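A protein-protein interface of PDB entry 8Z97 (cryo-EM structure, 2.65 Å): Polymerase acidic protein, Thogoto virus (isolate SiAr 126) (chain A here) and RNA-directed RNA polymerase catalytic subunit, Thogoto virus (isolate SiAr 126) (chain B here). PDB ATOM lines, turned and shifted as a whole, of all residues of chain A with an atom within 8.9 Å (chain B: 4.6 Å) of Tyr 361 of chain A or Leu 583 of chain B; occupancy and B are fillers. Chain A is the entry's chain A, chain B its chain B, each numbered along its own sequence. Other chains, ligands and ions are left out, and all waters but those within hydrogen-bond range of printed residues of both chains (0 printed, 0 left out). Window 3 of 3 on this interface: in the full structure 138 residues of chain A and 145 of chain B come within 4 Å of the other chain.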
ATOM      1  N   ASN A 358      -2.465  16.909 -23.650  1.00  0.00           N
ATOM      2  CA  ASN A 358      -1.180  17.434 -23.222  1.00  0.00           C
ATOM      3  C   ASN A 358      -1.275  17.956 -21.791  1.00  0.00           C
ATOM      4  O   ASN A 358      -2.359  18.127 -21.230  1.00  0.00           O
ATOM      5  CB  ASN A 358      -0.708  18.545 -24.158  1.00  0.00           C
ATOM      6  CG  ASN A 358      -0.705  18.123 -25.613  1.00  0.00           C
ATOM      7  OD1 ASN A 358      -1.169  18.859 -26.482  1.00  0.00           O
ATOM      8  ND2 ASN A 358      -0.176  16.936 -25.885  1.00  0.00           N
ATOM      9  N   ALA A 359      -0.113  18.208 -21.199  1.00  0.00           N
ATOM     10  CA  ALA A 359      -0.070  18.750 -19.852  1.00  0.00           C
ATOM     11  C   ALA A 359      -0.541  20.202 -19.845  1.00  0.00           C
ATOM     12  O   ALA A 359      -0.599  20.871 -20.879  1.00  0.00           O
ATOM     13  CB  ALA A 359       1.343  18.651 -19.281  1.00  0.00           C
ATOM     14  N   ILE A 360      -0.908  20.679 -18.659  1.00  0.00           N
ATOM     15  CA  ILE A 360      -1.347  22.056 -18.464  1.00  0.00           C
ATOM     16  C   ILE A 360      -0.518  22.662 -17.343  1.00  0.00           C
ATOM     17  O   ILE A 360      -0.476  22.116 -16.233  1.00  0.00           O
ATOM     18  CB  ILE A 360      -2.848  22.147 -18.139  1.00  0.00           C
ATOM     19  CG1 ILE A 360      -3.663  21.325 -19.138  1.00  0.00           C
ATOM     20  CG2 ILE A 360      -3.303  23.596 -18.138  1.00  0.00           C
ATOM     21  CD1 ILE A 360      -5.153  21.373 -18.895  1.00  0.00           C
ATOM     22  N   TYR A 361       0.134  23.788 -17.627  1.00  0.00           N
ATOM     23  CA  TYR A 361       0.950  24.469 -16.631  1.00  0.00           C
ATOM     24  C   TYR A 361       0.552  25.935 -16.521  1.00  0.00           C
ATOM     25  O   TYR A 361       0.686  26.543 -15.454  1.00  0.00           O
ATOM     26  CB  TYR A 361       2.435  24.348 -16.978  1.00  0.00           C
ATOM     27  CG  TYR A 361       2.907  22.925 -17.167  1.00  0.00           C
ATOM     28  CD1 TYR A 361       2.680  21.962 -16.195  1.00  0.00           C
ATOM     29  CD2 TYR A 361       3.579  22.545 -18.319  1.00  0.00           C
ATOM     30  CE1 TYR A 361       3.108  20.661 -16.367  1.00  0.00           C
ATOM     31  CE2 TYR A 361       4.011  21.249 -18.499  1.00  0.00           C
ATOM     32  CZ  TYR A 361       3.774  20.312 -17.520  1.00  0.00           C
ATOM     33  OH  TYR A 361       4.202  19.018 -17.699  1.00  0.00           O
ATOM     34  N   THR A 362       0.062  26.508 -17.615  1.00  0.00           N
ATOM     35  CA  THR A 362      -0.323  27.910 -17.671  1.00  0.00           C
ATOM     36  C   THR A 362      -1.771  28.033 -18.127  1.00  0.00           C
ATOM     37  O   THR A 362      -2.427  27.047 -18.475  1.00  0.00           O
ATOM     38  CB  THR A 362       0.597  28.698 -18.612  1.00  0.00           C
ATOM     39  OG1 THR A 362       0.488  28.175 -19.941  1.00  0.00           O
ATOM     40  CG2 THR A 362       2.042  28.597 -18.156  1.00  0.00           C
ATOM     41  N   GLU A 363      -2.273  29.271 -18.113  1.00  0.00           N
ATOM     42  CA  GLU A 363      -3.647  29.518 -18.538  1.00  0.00           C
ATOM     43  C   GLU A 363      -3.786  29.407 -20.052  1.00  0.00           C
ATOM     44  O   GLU A 363      -4.821  28.950 -20.555  1.00  0.00           O
ATOM     45  CB  GLU A 363      -4.102  30.893 -18.050  1.00  0.00           C
ATOM     46  CG  GLU A 363      -5.593  31.146 -18.193  1.00  0.00           C
ATOM     47  CD  GLU A 363      -5.954  32.609 -18.011  1.00  0.00           C
ATOM     48  OE1 GLU A 363      -5.138  33.355 -17.429  1.00  0.00           O
ATOM     49  OE2 GLU A 363      -7.052  33.011 -18.450  1.00  0.00           O
ATOM     50  N   VAL A 364      -2.757  29.827 -20.793  1.00  0.00           N
ATOM     51  CA  VAL A 364      -2.752  29.636 -22.241  1.00  0.00           C
ATOM     52  C   VAL A 364      -2.853  28.154 -22.571  1.00  0.00           C
ATOM     53  O   VAL A 364      -3.568  27.751 -23.498  1.00  0.00           O
ATOM     54  CB  VAL A 364      -1.489  30.264 -22.859  1.00  0.00           C
ATOM     55  CG1 VAL A 364      -1.435  29.996 -24.353  1.00  0.00           C
ATOM     56  CG2 VAL A 364      -1.441  31.753 -22.580  1.00  0.00           C
ATOM     57  N   ASP A 365      -2.145  27.322 -21.811  1.00  0.00           N
ATOM     58  CA  ASP A 365      -2.239  25.882 -21.996  1.00  0.00           C
ATOM     59  C   ASP A 365      -3.661  25.397 -21.754  1.00  0.00           C
ATOM     60  O   ASP A 365      -4.186  24.574 -22.515  1.00  0.00           O
ATOM     61  CB  ASP A 365      -1.266  25.185 -21.052  1.00  0.00           C
ATOM     62  CG  ASP A 365       0.176  25.434 -21.423  1.00  0.00           C
ATOM     63  OD1 ASP A 365       0.453  25.639 -22.622  1.00  0.00           O
ATOM     64  OD2 ASP A 365       1.034  25.423 -20.519  1.00  0.00           O
ATOM     65  N   GLY A 366      -4.304  25.911 -20.704  1.00  0.00           N
ATOM     66  CA  GLY A 366      -5.664  25.498 -20.407  1.00  0.00           C
ATOM     67  C   GLY A 366      -6.636  25.856 -21.512  1.00  0.00           C
ATOM     68  O   GLY A 366      -7.472  25.040 -21.907  1.00  0.00           O
ATOM     69  N   VAL A 367      -6.540  27.082 -22.033  1.00  0.00           N
ATOM     70  CA  VAL A 367      -7.465  27.487 -23.089  1.00  0.00           C
ATOM     71  C   VAL A 367      -7.185  26.713 -24.374  1.00  0.00           C
ATOM     72  O   VAL A 367      -8.113  26.363 -25.114  1.00  0.00           O
ATOM     73  CB  VAL A 367      -7.426  29.013 -23.308  1.00  0.00           C
ATOM     74  CG1 VAL A 367      -7.761  29.742 -22.014  1.00  0.00           C
ATOM     75  CG2 VAL A 367      -6.092  29.471 -23.853  1.00  0.00           C
ATOM     76  N   GLU A 369      -6.022  23.571 -24.589  1.00  0.00           N
ATOM     77  CA  GLU A 369      -6.598  22.240 -24.430  1.00  0.00           C
ATOM     78  C   GLU A 369      -8.120  22.280 -24.430  1.00  0.00           C
ATOM     79  O   GLU A 369      -8.756  21.346 -24.924  1.00  0.00           O
ATOM     80  CB  GLU A 369      -6.080  21.572 -23.158  1.00  0.00           C
ATOM     81  CG  GLU A 369      -4.574  21.622 -23.008  1.00  0.00           C
ATOM     82  CD  GLU A 369      -3.855  20.751 -24.019  1.00  0.00           C
ATOM     83  OE1 GLU A 369      -4.471  19.796 -24.537  1.00  0.00           O
ATOM     84  OE2 GLU A 369      -2.673  21.034 -24.307  1.00  0.00           O
ATOM     85  N   VAL B 566       4.672  15.060 -21.022  1.00  0.00           N
ATOM     86  CA  VAL B 566       5.108  16.070 -20.067  1.00  0.00           C
ATOM     87  C   VAL B 566       5.134  17.414 -20.779  1.00  0.00           C
ATOM     88  O   VAL B 566       5.012  18.469 -20.148  1.00  0.00           O
ATOM     89  CB  VAL B 566       6.481  15.719 -19.463  1.00  0.00           C
ATOM     90  CG1 VAL B 566       7.576  15.814 -20.515  1.00  0.00           C
ATOM     91  CG2 VAL B 566       6.790  16.614 -18.274  1.00  0.00           C
ATOM     92  N   SER B 568       3.809  20.489 -22.752  1.00  0.00           N
ATOM     93  CA  SER B 568       2.571  21.227 -22.907  1.00  0.00           C
ATOM     94  C   SER B 568       2.709  22.184 -24.084  1.00  0.00           C
ATOM     95  O   SER B 568       3.743  22.234 -24.755  1.00  0.00           O
ATOM     96  CB  SER B 568       2.229  21.967 -21.617  1.00  0.00           C
ATOM     97  OG  SER B 568       1.084  22.771 -21.796  1.00  0.00           O
ATOM     98  N   THR B 571       5.366  24.644 -23.226  1.00  0.00           N
ATOM     99  CA  THR B 571       6.665  24.044 -22.946  1.00  0.00           C
ATOM    100  C   THR B 571       7.171  23.217 -24.125  1.00  0.00           C
ATOM    101  O   THR B 571       7.852  22.210 -23.937  1.00  0.00           O
ATOM    102  CB  THR B 571       6.607  23.185 -21.684  1.00  0.00           C
ATOM    103  OG1 THR B 571       5.654  22.131 -21.865  1.00  0.00           O
ATOM    104  CG2 THR B 571       6.204  24.023 -20.486  1.00  0.00           C
ATOM    105  N   LEU B 579      12.662  18.565 -18.053  1.00  0.00           N
ATOM    106  CA  LEU B 579      11.351  18.970 -17.556  1.00  0.00           C
ATOM    107  C   LEU B 579      10.768  17.925 -16.613  1.00  0.00           C
ATOM    108  O   LEU B 579      10.202  18.269 -15.568  1.00  0.00           O
ATOM    109  CB  LEU B 579      10.409  19.228 -18.731  1.00  0.00           C
ATOM    110  CG  LEU B 579       8.974  19.644 -18.413  1.00  0.00           C
ATOM    111  CD1 LEU B 579       8.959  20.902 -17.565  1.00  0.00           C
ATOM    112  CD2 LEU B 579       8.192  19.851 -19.696  1.00  0.00           C
ATOM    113  N   ARG B 580      10.899  16.642 -16.962  1.00  0.00           N
ATOM    114  CA  ARG B 580      10.416  15.583 -16.083  1.00  0.00           C
ATOM    115  C   ARG B 580      11.171  15.578 -14.762  1.00  0.00           C
ATOM    116  O   ARG B 580      10.576  15.358 -13.700  1.00  0.00           O
ATOM    117  CB  ARG B 580      10.536  14.225 -16.775  1.00  0.00           C
ATOM    118  CG  ARG B 580       9.591  14.042 -17.947  1.00  0.00           C
ATOM    119  CD  ARG B 580       9.581  12.605 -18.433  1.00  0.00           C
ATOM    120  NE  ARG B 580       8.560  12.383 -19.449  1.00  0.00           N
ATOM    121  CZ  ARG B 580       7.285  12.136 -19.186  1.00  0.00           C
ATOM    122  NH1 ARG B 580       6.834  12.073 -17.945  1.00  0.00           N
ATOM    123  NH2 ARG B 580       6.440  11.948 -20.195  1.00  0.00           N
ATOM    124  N   ARG B 581      12.485  15.813 -14.804  1.00  0.00           N
ATOM    125  CA  ARG B 581      13.257  15.899 -13.570  1.00  0.00           C
ATOM    126  C   ARG B 581      12.792  17.065 -12.709  1.00  0.00           C
ATOM    127  O   ARG B 581      12.648  16.927 -11.489  1.00  0.00           O
ATOM    128  CB  ARG B 581      14.744  16.036 -13.887  1.00  0.00           C
ATOM    129  CG  ARG B 581      15.595  16.350 -12.671  1.00  0.00           C
ATOM    130  CD  ARG B 581      16.906  17.000 -13.063  1.00  0.00           C
ATOM    131  NE  ARG B 581      17.932  16.797 -12.048  1.00  0.00           N
ATOM    132  CZ  ARG B 581      19.117  17.390 -12.053  1.00  0.00           C
ATOM    133  NH1 ARG B 581      19.461  18.240 -13.007  1.00  0.00           N
ATOM    134  NH2 ARG B 581      19.979  17.126 -11.076  1.00  0.00           N
ATOM    135  N   HIS B 582      12.553  18.223 -13.329  1.00  0.00           N
ATOM    136  CA  HIS B 582      12.102  19.386 -12.572  1.00  0.00           C
ATOM    137  C   HIS B 582      10.737  19.144 -11.942  1.00  0.00           C
ATOM    138  O   HIS B 582      10.497  19.538 -10.794  1.00  0.00           O
ATOM    139  CB  HIS B 582      12.059  20.617 -13.472  1.00  0.00           C
ATOM    140  CG  HIS B 582      11.421  21.810 -12.832  1.00  0.00           C
ATOM    141  ND1 HIS B 582      12.120  22.690 -12.035  1.00  0.00           N
ATOM    142  CD2 HIS B 582      10.148  22.267 -12.868  1.00  0.00           C
ATOM    143  CE1 HIS B 582      11.304  23.638 -11.609  1.00  0.00           C
ATOM    144  NE2 HIS B 582      10.102  23.404 -12.101  1.00  0.00           N
ATOM    145  N   LEU B 583       9.832  18.500 -12.672  1.00  0.00           N
ATOM    146  CA  LEU B 583       8.482  18.273 -12.175  1.00  0.00           C
ATOM    147  C   LEU B 583       8.384  17.092 -11.220  1.00  0.00           C
ATOM    148  O   LEU B 583       7.300  16.839 -10.685  1.00  0.00           O
ATOM    149  CB  LEU B 583       7.520  18.070 -13.347  1.00  0.00           C
ATOM    150  CG  LEU B 583       7.295  19.306 -14.216  1.00  0.00           C
ATOM    151  CD1 LEU B 583       6.432  18.958 -15.409  1.00  0.00           C
ATOM    152  CD2 LEU B 583       6.661  20.419 -13.402  1.00  0.00           C
ATOM    153  N   GLY B 584       9.476  16.366 -10.993  1.00  0.00           N
ATOM    154  CA  GLY B 584       9.461  15.233 -10.096  1.00  0.00           C
ATOM    155  C   GLY B 584       8.929  13.950 -10.691  1.00  0.00           C
ATOM    156  O   GLY B 584       8.826  12.950  -9.971  1.00  0.00           O
ATOM    157  N   LEU B 585       8.588  13.944 -11.979  1.00  0.00           N
ATOM    158  CA  LEU B 585       8.090  12.743 -12.636  1.00  0.00           C
ATOM    159  C   LEU B 585       9.186  11.730 -12.927  1.00  0.00           C
ATOM    160  O   LEU B 585       8.873  10.597 -13.309  1.00  0.00           O
ATOM    161  CB  LEU B 585       7.381  13.115 -13.939  1.00  0.00           C
ATOM    162  CG  LEU B 585       6.254  14.140 -13.814  1.00  0.00           C
ATOM    163  CD1 LEU B 585       5.876  14.686 -15.177  1.00  0.00           C
ATOM    164  CD2 LEU B 585       5.049  13.521 -13.128  1.00  0.00           C
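Hydrophobic or aromatic side chains of chain A that line the printed part of chain B: Ala 359 and Tyr 361. Of the 10 printed residues of chain B, 4 touch a printed residue of chain A. Among the printed residues, 7 pairs touch across the chains.
Tyr 361 of chain A touches just these residues of chain B: Val 566 (2.6 Å), Ser 568 (3.6 Å), Thr 571 (3.7 Å) and Leu 583 (3.2 Å). Glu 363 of chain A touches none of the printed residues of chain B. Of the printed residues of chain A, Ser 568 of chain B touches Ala 359 (2.7 Å), Tyr 361 (3.6 Å) and Asp 365 (2.8 Å). Of the printed residues of chain A, Thr 571 of chain B touches Tyr 361 (3.7 Å). Of the printed residues of chain A, Leu 583 of chain B touches Tyr 361. No residue of chain A comes within 4 Å of Gly 584 of chain B. The nearest residue of chain B that does not touch Tyr 361 of chain A is Leu 579 of chain B (4.5 Å). The nearest residue of chain A that does not touch Leu 583 of chain B is Ala 359 of chain A (6.4 Å).
Among the printed residues, pairs that only touch across the chains: Ala 359 of chain A with Val 566 of chain B, Tyr 361 of chain A with Ser 568 of chain B, Tyr 361 of chain A with Thr 571 of chain B and Tyr 361 of chain A with Leu 583 of chain B.
The backbone NH of Tyr 361 of chain A is in hydrogen-bond range of the side-chain carboxylate of Asp 365 of chain A (3.4 Å). The side-chain hydroxyl (OG1) of Thr 362 of chain A lies within hydrogen-bond range of the side-chain carboxylate (OD2) of Asp 365 of chain A (2.9 Å). N of Ser 568 of chain B sits at hydrogen-bond distance from OG1 of Thr 571 of chain B, at 2.6 Å.
O of Ala 359 of chain A lies within hydrogen-bond range of OG of Ser 568 of chain B (2.7 Å). The backbone carbonyl oxygen of Val 566 of chain B sits at hydrogen-bond distance from the side-chain hydroxyl of Tyr 361 of chain A. The side-chain carboxylate of Asp 365 of chain A lies close to the side-chain hydroxyl of Ser 568 of chain B (2.9 Å).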
